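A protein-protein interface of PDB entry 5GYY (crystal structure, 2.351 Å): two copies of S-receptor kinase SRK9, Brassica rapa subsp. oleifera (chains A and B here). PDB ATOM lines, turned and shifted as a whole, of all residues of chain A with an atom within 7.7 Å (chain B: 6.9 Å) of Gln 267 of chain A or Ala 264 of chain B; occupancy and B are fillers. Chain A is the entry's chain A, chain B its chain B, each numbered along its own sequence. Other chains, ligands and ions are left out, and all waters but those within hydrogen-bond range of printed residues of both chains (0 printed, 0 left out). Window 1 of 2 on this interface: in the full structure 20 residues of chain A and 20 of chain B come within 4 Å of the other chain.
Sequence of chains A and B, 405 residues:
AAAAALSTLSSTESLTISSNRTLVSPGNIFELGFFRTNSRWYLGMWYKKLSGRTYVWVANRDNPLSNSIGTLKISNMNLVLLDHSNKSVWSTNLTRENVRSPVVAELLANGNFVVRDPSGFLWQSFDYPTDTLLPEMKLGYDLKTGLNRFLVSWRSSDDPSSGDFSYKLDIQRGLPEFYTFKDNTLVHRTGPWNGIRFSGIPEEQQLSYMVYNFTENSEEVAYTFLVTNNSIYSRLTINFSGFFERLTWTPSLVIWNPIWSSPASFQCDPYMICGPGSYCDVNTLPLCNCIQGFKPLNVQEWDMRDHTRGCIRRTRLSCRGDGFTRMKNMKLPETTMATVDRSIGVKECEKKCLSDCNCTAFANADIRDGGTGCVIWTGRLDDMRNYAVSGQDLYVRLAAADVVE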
ATOM      1  N   PRO A 263      27.389   9.683   3.399  1.00  0.00           N
ATOM      2  CA  PRO A 263      26.401   9.722   4.489  1.00  0.00           C
ATOM      3  C   PRO A 263      26.964   9.263   5.828  1.00  0.00           C
ATOM      4  O   PRO A 263      27.702   8.277   5.877  1.00  0.00           O
ATOM      5  CB  PRO A 263      25.319   8.737   4.029  1.00  0.00           C
ATOM      6  CG  PRO A 263      25.958   7.888   3.029  1.00  0.00           C
ATOM      7  CD  PRO A 263      27.036   8.689   2.377  1.00  0.00           C
ATOM      8  N   ALA A 264      26.591   9.961   6.895  1.00  0.00           N
ATOM      9  CA  ALA A 264      27.134   9.710   8.224  1.00  0.00           C
ATOM     10  C   ALA A 264      26.389   8.609   8.954  1.00  0.00           C
ATOM     11  O   ALA A 264      26.920   8.017   9.873  1.00  0.00           O
ATOM     12  CB  ALA A 264      27.106  10.992   9.053  1.00  0.00           C
ATOM     13  N   SER A 265      25.142   8.371   8.571  1.00  0.00           N
ATOM     14  CA  SER A 265      24.307   7.392   9.256  1.00  0.00           C
ATOM     15  C   SER A 265      23.548   6.543   8.254  1.00  0.00           C
ATOM     16  O   SER A 265      22.803   7.082   7.424  1.00  0.00           O
ATOM     17  CB  SER A 265      23.307   8.097  10.166  1.00  0.00           C
ATOM     18  OG  SER A 265      22.299   7.191  10.585  1.00  0.00           O
ATOM     19  N   PHE A 266      23.757   5.229   8.306  1.00  0.00           N
ATOM     20  CA  PHE A 266      23.037   4.298   7.443  1.00  0.00           C
ATOM     21  C   PHE A 266      21.578   4.248   7.858  1.00  0.00           C
ATOM     22  O   PHE A 266      20.718   3.830   7.079  1.00  0.00           O
ATOM     23  CB  PHE A 266      23.619   2.892   7.533  1.00  0.00           C
ATOM     24  CG  PHE A 266      24.959   2.737   6.856  1.00  0.00           C
ATOM     25  CD1 PHE A 266      25.413   3.684   5.947  1.00  0.00           C
ATOM     26  CD2 PHE A 266      25.749   1.616   7.099  1.00  0.00           C
ATOM     27  CE1 PHE A 266      26.648   3.534   5.327  1.00  0.00           C
ATOM     28  CE2 PHE A 266      26.977   1.461   6.471  1.00  0.00           C
ATOM     29  CZ  PHE A 266      27.424   2.421   5.587  1.00  0.00           C
ATOM     30  N   GLN A 267      21.312   4.648   9.100  1.00  0.00           N
ATOM     31  CA  GLN A 267      19.953   4.654   9.633  1.00  0.00           C
ATOM     32  C   GLN A 267      19.069   5.743   9.006  1.00  0.00           C
ATOM     33  O   GLN A 267      17.956   5.451   8.584  1.00  0.00           O
ATOM     34  CB  GLN A 267      19.950   4.844  11.156  1.00  0.00           C
ATOM     35  CG  GLN A 267      20.562   3.697  11.967  1.00  0.00           C
ATOM     36  CD  GLN A 267      22.078   3.766  12.027  1.00  0.00           C
ATOM     37  OE1 GLN A 267      22.677   4.810  11.764  1.00  0.00           O
ATOM     38  NE2 GLN A 267      22.704   2.661  12.400  1.00  0.00           N
ATOM     39  N   CYS A 268      19.558   6.986   8.947  1.00  0.00           N
ATOM     40  CA  CYS A 268      18.695   8.121   8.577  1.00  0.00           C
ATOM     41  C   CYS A 268      19.090   8.935   7.348  1.00  0.00           C
ATOM     42  O   CYS A 268      18.261   9.652   6.785  1.00  0.00           O
ATOM     43  CB  CYS A 268      18.505   9.060   9.768  1.00  0.00           C
ATOM     44  SG  CYS A 268      17.304   8.447  10.957  1.00  0.00           S
ATOM     45  N   ASP A 269      20.348   8.838   6.933  1.00  0.00           N
ATOM     46  CA  ASP A 269      20.826   9.616   5.786  1.00  0.00           C
ATOM     47  C   ASP A 269      20.474   9.084   4.389  1.00  0.00           C
ATOM     48  O   ASP A 269      20.315   9.888   3.463  1.00  0.00           O
ATOM     49  CB  ASP A 269      22.330   9.872   5.877  1.00  0.00           C
ATOM     50  CG  ASP A 269      22.685  10.946   6.893  1.00  0.00           C
ATOM     51  OD1 ASP A 269      21.872  11.876   7.102  1.00  0.00           O
ATOM     52  OD2 ASP A 269      23.781  10.851   7.487  1.00  0.00           O
ATOM     53  N   PRO A 270      20.356   7.747   4.214  1.00  0.00           N
ATOM     54  CA  PRO A 270      20.000   7.324   2.848  1.00  0.00           C
ATOM     55  C   PRO A 270      18.726   7.968   2.269  1.00  0.00           C
ATOM     56  O   PRO A 270      17.753   8.234   2.970  1.00  0.00           O
ATOM     57  CB  PRO A 270      19.842   5.805   2.988  1.00  0.00           C
ATOM     58  CG  PRO A 270      20.798   5.447   4.050  1.00  0.00           C
ATOM     59  CD  PRO A 270      20.764   6.594   5.040  1.00  0.00           C
ATOM     60  N   ILE A 273      14.744   6.944   3.165  1.00  0.00           N
ATOM     61  CA  ILE A 273      14.511   5.741   3.980  1.00  0.00           C
ATOM     62  C   ILE A 273      13.133   5.808   4.630  1.00  0.00           C
ATOM     63  O   ILE A 273      12.543   4.773   4.929  1.00  0.00           O
ATOM     64  CB  ILE A 273      15.583   5.461   5.072  1.00  0.00           C
ATOM     65  CG1 ILE A 273      16.473   6.677   5.303  1.00  0.00           C
ATOM     66  CG2 ILE A 273      16.381   4.182   4.748  1.00  0.00           C
ATOM     67  CD1 ILE A 273      15.769   7.806   6.028  1.00  0.00           C
ATOM     68  N   CYS A 274      12.630   7.026   4.847  1.00  0.00           N
ATOM     69  CA  CYS A 274      11.255   7.241   5.311  1.00  0.00           C
ATOM     70  C   CYS A 274      10.381   7.802   4.191  1.00  0.00           C
ATOM     71  O   CYS A 274      10.843   8.596   3.373  1.00  0.00           O
ATOM     72  CB  CYS A 274      11.225   8.189   6.520  1.00  0.00           C
ATOM     73  SG  CYS A 274      12.202   7.623   7.930  1.00  0.00           S
ATOM     74  N   CYS A 280      13.072  10.917   9.502  1.00  0.00           N
ATOM     75  CA  CYS A 280      13.911   9.973  10.196  1.00  0.00           C
ATOM     76  C   CYS A 280      14.543  10.618  11.438  1.00  0.00           C
ATOM     77  O   CYS A 280      15.012  11.754  11.399  1.00  0.00           O
ATOM     78  CB  CYS A 280      14.984   9.445   9.230  1.00  0.00           C
ATOM     79  SG  CYS A 280      15.757   7.897   9.752  1.00  0.00           S
ATOM     80  N   ASP A 281      14.559   9.875  12.541  1.00  0.00           N
ATOM     81  CA  ASP A 281      15.148  10.333  13.799  1.00  0.00           C
ATOM     82  C   ASP A 281      15.975   9.172  14.369  1.00  0.00           C
ATOM     83  O   ASP A 281      15.404   8.137  14.741  1.00  0.00           O
ATOM     84  CB  ASP A 281      14.036  10.737  14.776  1.00  0.00           C
ATOM     85  CG  ASP A 281      14.577  11.354  16.088  1.00  0.00           C
ATOM     86  OD1 ASP A 281      15.745  11.083  16.461  1.00  0.00           O
ATOM     87  OD2 ASP A 281      13.812  12.068  16.785  1.00  0.00           O
ATOM     88  N   VAL A 282      17.298   9.350  14.472  1.00  0.00           N
ATOM     89  CA  VAL A 282      18.163   8.246  14.878  1.00  0.00           C
ATOM     90  C   VAL A 282      17.946   7.783  16.312  1.00  0.00           C
ATOM     91  O   VAL A 282      18.368   6.690  16.690  1.00  0.00           O
ATOM     92  CB  VAL A 282      19.680   8.515  14.656  1.00  0.00           C
ATOM     93  CG1 VAL A 282      20.024   8.522  13.172  1.00  0.00           C
ATOM     94  CG2 VAL A 282      20.146   9.776  15.340  1.00  0.00           C
ATOM     95  N   ASN A 283      17.264   8.598  17.102  1.00  0.00           N
ATOM     96  CA  ASN A 283      17.089   8.296  18.512  1.00  0.00           C
ATOM     97  C   ASN A 283      15.706   7.783  18.871  1.00  0.00           C
ATOM     98  O   ASN A 283      15.319   7.789  20.036  1.00  0.00           O
ATOM     99  CB  ASN A 283      17.427   9.524  19.351  1.00  0.00           C
ATOM    100  CG  ASN A 283      18.829  10.035  19.093  1.00  0.00           C
ATOM    101  OD1 ASN A 283      19.790   9.274  19.104  1.00  0.00           O
ATOM    102  ND2 ASN A 283      18.949  11.333  18.849  1.00  0.00           N
ATOM    103  N   LEU A 287      12.476   4.338  13.364  1.00  0.00           N
ATOM    104  CA  LEU A 287      13.302   5.458  12.917  1.00  0.00           C
ATOM    105  C   LEU A 287      12.421   6.535  12.277  1.00  0.00           C
ATOM    106  O   LEU A 287      12.685   7.733  12.393  1.00  0.00           O
ATOM    107  CB  LEU A 287      14.388   4.984  11.937  1.00  0.00           C
ATOM    108  CG  LEU A 287      15.516   4.080  12.465  1.00  0.00           C
ATOM    109  CD1 LEU A 287      16.350   3.461  11.323  1.00  0.00           C
ATOM    110  CD2 LEU A 287      16.416   4.882  13.384  1.00  0.00           C
ATOM    111  N   CYS A 288      11.365   6.099  11.607  1.00  0.00           N
ATOM    112  CA  CYS A 288      10.515   7.014  10.857  1.00  0.00           C
ATOM    113  C   CYS A 288       9.339   7.489  11.692  1.00  0.00           C
ATOM    114  O   CYS A 288       8.558   6.674  12.194  1.00  0.00           O
ATOM    115  CB  CYS A 288      10.014   6.344   9.580  1.00  0.00           C
ATOM    116  SG  CYS A 288      11.327   5.862   8.466  1.00  0.00           S
ATOM    117  N   ARG A 385      14.813  14.262   7.668  1.00  0.00           N
ATOM    118  CA  ARG A 385      15.338  13.704   8.889  1.00  0.00           C
ATOM    119  C   ARG A 385      15.610  14.855   9.832  1.00  0.00           C
ATOM    120  O   ARG A 385      15.732  15.998   9.388  1.00  0.00           O
ATOM    121  CB  ARG A 385      16.625  12.931   8.607  1.00  0.00           C
ATOM    122  CG  ARG A 385      17.843  13.800   8.301  1.00  0.00           C
ATOM    123  CD  ARG A 385      19.150  13.041   8.591  1.00  0.00           C
ATOM    124  NE  ARG A 385      19.434  12.964  10.024  1.00  0.00           N
ATOM    125  CZ  ARG A 385      20.497  12.360  10.556  1.00  0.00           C
ATOM    126  NH1 ARG A 385      21.391  11.765   9.773  1.00  0.00           N
ATOM    127  NH2 ARG A 385      20.677  12.362  11.875  1.00  0.00           N
ATOM    128  N   HIS B 188      34.878  -4.027  18.054  1.00  0.00           N
ATOM    129  CA  HIS B 188      33.722  -3.408  18.685  1.00  0.00           C
ATOM    130  C   HIS B 188      33.360  -4.129  19.996  1.00  0.00           C
ATOM    131  O   HIS B 188      33.502  -5.352  20.120  1.00  0.00           O
ATOM    132  CB  HIS B 188      32.520  -3.369  17.732  1.00  0.00           C
ATOM    133  CG  HIS B 188      31.268  -2.853  18.367  1.00  0.00           C
ATOM    134  ND1 HIS B 188      30.211  -3.672  18.696  1.00  0.00           N
ATOM    135  CD2 HIS B 188      30.926  -1.611  18.787  1.00  0.00           C
ATOM    136  CE1 HIS B 188      29.263  -2.956  19.273  1.00  0.00           C
ATOM    137  NE2 HIS B 188      29.672  -1.702  19.339  1.00  0.00           N
ATOM    138  N   GLY B 200      25.936  -1.467  24.807  1.00  0.00           N
ATOM    139  CA  GLY B 200      26.331  -0.930  23.517  1.00  0.00           C
ATOM    140  C   GLY B 200      25.406  -1.190  22.343  1.00  0.00           C
ATOM    141  O   GLY B 200      25.769  -0.893  21.204  1.00  0.00           O
ATOM    142  N   PRO B 202      21.624  -0.124  22.089  1.00  0.00           N
ATOM    143  CA  PRO B 202      20.397   0.449  22.669  1.00  0.00           C
ATOM    144  C   PRO B 202      19.115   0.210  21.858  1.00  0.00           C
ATOM    145  O   PRO B 202      18.021   0.410  22.412  1.00  0.00           O
ATOM    146  CB  PRO B 202      20.714   1.950  22.782  1.00  0.00           C
ATOM    147  CG  PRO B 202      21.828   2.200  21.816  1.00  0.00           C
ATOM    148  CD  PRO B 202      22.597   0.909  21.677  1.00  0.00           C
ATOM    149  N   GLU B 203      19.234  -0.243  20.605  1.00  0.00           N
ATOM    150  CA  GLU B 203      18.048  -0.468  19.783  1.00  0.00           C
ATOM    151  C   GLU B 203      17.285  -1.731  20.151  1.00  0.00           C
ATOM    152  O   GLU B 203      16.081  -1.822  19.898  1.00  0.00           O
ATOM    153  CB  GLU B 203      18.386  -0.494  18.280  1.00  0.00           C
ATOM    154  CG  GLU B 203      19.084   0.761  17.734  1.00  0.00           C
ATOM    155  CD  GLU B 203      20.579   0.757  18.065  1.00  0.00           C
ATOM    156  OE1 GLU B 203      21.005  -0.120  18.854  1.00  0.00           O
ATOM    157  OE2 GLU B 203      21.322   1.632  17.566  1.00  0.00           O
ATOM    158  N   PHE B 243      28.965  -6.836  10.752  1.00  0.00           N
ATOM    159  CA  PHE B 243      27.861  -6.238  11.491  1.00  0.00           C
ATOM    160  C   PHE B 243      26.971  -7.302  12.090  1.00  0.00           C
ATOM    161  O   PHE B 243      26.549  -8.238  11.411  1.00  0.00           O
ATOM    162  CB  PHE B 243      27.028  -5.274  10.629  1.00  0.00           C
ATOM    163  CG  PHE B 243      27.789  -4.077  10.144  1.00  0.00           C
ATOM    164  CD1 PHE B 243      27.875  -2.934  10.926  1.00  0.00           C
ATOM    165  CD2 PHE B 243      28.417  -4.091   8.898  1.00  0.00           C
ATOM    166  CE1 PHE B 243      28.586  -1.806  10.480  1.00  0.00           C
ATOM    167  CE2 PHE B 243      29.128  -2.981   8.448  1.00  0.00           C
ATOM    168  CZ  PHE B 243      29.209  -1.836   9.241  1.00  0.00           C
ATOM    169  N   TRP B 260      17.951  -3.672  13.738  1.00  0.00           N
ATOM    170  CA  TRP B 260      19.109  -2.893  14.168  1.00  0.00           C
ATOM    171  C   TRP B 260      20.415  -3.480  13.641  1.00  0.00           C
ATOM    172  O   TRP B 260      20.462  -4.640  13.214  1.00  0.00           O
ATOM    173  CB  TRP B 260      19.161  -2.709  15.700  1.00  0.00           C
ATOM    174  CG  TRP B 260      19.001  -3.956  16.557  1.00  0.00           C
ATOM    175  CD1 TRP B 260      17.889  -4.328  17.260  1.00  0.00           C
ATOM    176  CD2 TRP B 260      19.998  -4.964  16.830  1.00  0.00           C
ATOM    177  NE1 TRP B 260      18.126  -5.503  17.935  1.00  0.00           N
ATOM    178  CE2 TRP B 260      19.409  -5.913  17.685  1.00  0.00           C
ATOM    179  CE3 TRP B 260      21.322  -5.156  16.422  1.00  0.00           C
ATOM    180  CZ2 TRP B 260      20.100  -7.037  18.145  1.00  0.00           C
ATOM    181  CZ3 TRP B 260      22.005  -6.272  16.878  1.00  0.00           C
ATOM    182  CH2 TRP B 260      21.393  -7.198  17.727  1.00  0.00           C
ATOM    183  N   SER B 261      21.473  -2.676  13.677  1.00  0.00           N
ATOM    184  CA  SER B 261      22.769  -3.094  13.157  1.00  0.00           C
ATOM    185  C   SER B 261      23.846  -2.573  14.044  1.00  0.00           C
ATOM    186  O   SER B 261      23.802  -1.412  14.447  1.00  0.00           O
ATOM    187  CB  SER B 261      22.986  -2.595  11.731  1.00  0.00           C
ATOM    188  OG  SER B 261      22.080  -3.258  10.876  1.00  0.00           O
ATOM    189  N   SER B 262      24.811  -3.440  14.358  1.00  0.00           N
ATOM    190  CA  SER B 262      25.862  -3.085  15.298  1.00  0.00           C
ATOM    191  C   SER B 262      27.236  -3.470  14.740  1.00  0.00           C
ATOM    192  O   SER B 262      27.447  -4.615  14.340  1.00  0.00           O
ATOM    193  CB  SER B 262      25.584  -3.780  16.642  1.00  0.00           C
ATOM    194  OG  SER B 262      26.465  -3.339  17.647  1.00  0.00           O
ATOM    195  N   PRO B 263      28.190  -2.525  14.732  1.00  0.00           N
ATOM    196  CA  PRO B 263      28.101  -1.142  15.231  1.00  0.00           C
ATOM    197  C   PRO B 263      27.179  -0.242  14.410  1.00  0.00           C
ATOM    198  O   PRO B 263      27.121  -0.363  13.190  1.00  0.00           O
ATOM    199  CB  PRO B 263      29.545  -0.624  15.129  1.00  0.00           C
ATOM    200  CG  PRO B 263      30.235  -1.542  14.178  1.00  0.00           C
ATOM    201  CD  PRO B 263      29.553  -2.877  14.293  1.00  0.00           C
ATOM    202  N   ALA B 264      26.454   0.626  15.111  1.00  0.00           N
ATOM    203  CA  ALA B 264      25.474   1.524  14.531  1.00  0.00           C
ATOM    204  C   ALA B 264      26.122   2.812  14.036  1.00  0.00           C
ATOM    205  O   ALA B 264      25.619   3.440  13.116  1.00  0.00           O
ATOM    206  CB  ALA B 264      24.382   1.848  15.561  1.00  0.00           C
ATOM    207  N   SER B 265      27.257   3.179  14.625  1.00  0.00           N
ATOM    208  CA  SER B 265      27.907   4.454  14.317  1.00  0.00           C
ATOM    209  C   SER B 265      29.417   4.311  14.094  1.00  0.00           C
ATOM    210  O   SER B 265      30.150   3.935  15.006  1.00  0.00           O
ATOM    211  CB  SER B 265      27.662   5.416  15.489  1.00  0.00           C
ATOM    212  OG  SER B 265      28.504   6.559  15.414  1.00  0.00           O
ATOM    213  N   PHE B 266      29.890   4.637  12.897  1.00  0.00           N
ATOM    214  CA  PHE B 266      31.323   4.581  12.586  1.00  0.00           C
ATOM    215  C   PHE B 266      32.047   5.644  13.406  1.00  0.00           C
ATOM    216  O   PHE B 266      33.251   5.559  13.631  1.00  0.00           O
ATOM    217  CB  PHE B 266      31.579   4.898  11.107  1.00  0.00           C
ATOM    218  CG  PHE B 266      31.172   3.818  10.146  1.00  0.00           C
ATOM    219  CD1 PHE B 266      31.011   2.508  10.555  1.00  0.00           C
ATOM    220  CD2 PHE B 266      30.948   4.126   8.807  1.00  0.00           C
ATOM    221  CE1 PHE B 266      30.638   1.518   9.644  1.00  0.00           C
ATOM    222  CE2 PHE B 266      30.576   3.140   7.896  1.00  0.00           C
ATOM    223  CZ  PHE B 266      30.424   1.831   8.323  1.00  0.00           C
ATOM    224  N   GLN B 267      31.308   6.672  13.809  1.00  0.00           N
ATOM    225  CA  GLN B 267      31.874   7.786  14.560  1.00  0.00           C
ATOM    226  C   GLN B 267      32.235   7.419  16.001  1.00  0.00           C
ATOM    227  O   GLN B 267      33.314   7.759  16.474  1.00  0.00           O
ATOM    228  CB  GLN B 267      30.916   8.979  14.580  1.00  0.00           C
ATOM    229  CG  GLN B 267      30.665   9.627  13.236  1.00  0.00           C
ATOM    230  CD  GLN B 267      29.639   8.868  12.426  1.00  0.00           C
ATOM    231  OE1 GLN B 267      28.875   8.066  12.969  1.00  0.00           O
ATOM    232  NE2 GLN B 267      29.606   9.123  11.121  1.00  0.00           N
ATOM    233  N   ASP B 269      31.089   4.184  17.833  1.00  0.00           N
ATOM    234  CA  ASP B 269      31.046   2.799  18.241  1.00  0.00           C
ATOM    235  C   ASP B 269      32.342   1.983  18.101  1.00  0.00           C
ATOM    236  O   ASP B 269      32.536   1.052  18.879  1.00  0.00           O
ATOM    237  CB  ASP B 269      29.889   2.068  17.572  1.00  0.00           C
ATOM    238  CG  ASP B 269      28.543   2.456  18.146  1.00  0.00           C
ATOM    239  OD1 ASP B 269      28.476   2.861  19.335  1.00  0.00           O
ATOM    240  OD2 ASP B 269      27.541   2.334  17.406  1.00  0.00           O
ATOM    241  N   ARG B 385      31.397   6.050  25.402  1.00  0.00           N
ATOM    242  CA  ARG B 385      30.651   6.948  24.533  1.00  0.00           C
ATOM    243  C   ARG B 385      29.360   7.313  25.264  1.00  0.00           C
ATOM    244  O   ARG B 385      28.996   6.671  26.246  1.00  0.00           O
ATOM    245  CB  ARG B 385      30.342   6.288  23.185  1.00  0.00           C
ATOM    246  CG  ARG B 385      29.276   5.194  23.238  1.00  0.00           C
ATOM    247  CD  ARG B 385      28.594   5.045  21.885  1.00  0.00           C
ATOM    248  NE  ARG B 385      27.587   6.081  21.601  1.00  0.00           N
ATOM    249  CZ  ARG B 385      26.894   6.152  20.463  1.00  0.00           C
ATOM    250  NH1 ARG B 385      27.122   5.274  19.482  1.00  0.00           N
ATOM    251  NH2 ARG B 385      25.983   7.108  20.286  1.00  0.00           N
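O of Ala 264 of chain A sits at hydrogen-bond distance from NE2 of Gln 267 of chain B (3.2 Å). The backbone carbonyl oxygen (O) of Ala 264 of chain B is in hydrogen-bond range of the side-chain amide nitrogen (NE2) of Gln 267 of chain A (3.1 Å).
The side-chain carboxylate of Asp 269 of chain A is in hydrogen-bond range of the backbone NH of Ala 264 of chain A (3.0 Å). The side-chain hydroxyl (OG) of Ser 265 of chain A lies within hydrogen-bond range of the side-chain amide oxygen (OE1) of Gln 267 of chain A (2.7 Å). The backbone NH of Ala 264 of chain B lies within hydrogen-bond range of the side-chain carboxylate of Asp 269 of chain B, 3.1 Å away. OE1 of Gln 267 of chain B lies within hydrogen-bond range of OG of Ser 265 of chain B (2.9 Å). SG of Cys 268 of chain A is disulfide-bonded to SG of Cys 280 of chain A, at 2.0 Å. The side-chain sulfur (SG) of Cys 274 of chain A is disulfide-bonded to the side-chain sulfur (SG) of Cys 288 of chain A (2.0 Å).
Among the printed residues, merely in contact across the chains: Phe 266 of chain A with Phe 266 of chain B (3.9 Å).
Printed residues of chain B within 4 Å of Ala 264 of chain A: Gln 267. Of the printed residues of chain B, Phe 266 of chain A touches Phe 266 (3.9 Å). Printed residues of chain B within 4 Å of Gln 267 of chain A: Ala 264. Asp 281 of chain A touches none of the printed residues of chain B. Ser 265 of chain B touches none of the printed residues of chain A. Printed residues of chain A within 4 Å of Phe 266 of chain B: Phe 266 (3.9 Å). Of the printed residues of chain A, Gln 267 of chain B touches Ala 264. The nearest residue of chain B that does not touch Gln 267 of chain A is Ser 261 of chain B (4.7 Å). The nearest residue of chain A that does not touch Ala 264 of chain B is Phe 266 of chain A (5.5 Å). The nearest printed residue of chain B that does not touch Ala 264 of chain A is Phe 266 of chain B (5.4 Å).
Of the 17 printed residues of chain A, 3 touch a printed residue of chain B. Hydrophobic or aromatic side chains of chain A within 4 Å of the printed part of chain B: Ala 264 and Phe 266. Printed residues of chain B that touch a printed residue of chain A: Ala 264, Phe 266 and Gln 267. Among the printed residues, 3 pairs touch across the chains.
Ala 264 of chain A touches Gln 267 of chain B, and with the chains exchanged Gln 267 of chain A touches Ala 264 of chain B. Phe 266 of chain B touches its own counterpart, Phe 266 of chain A.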
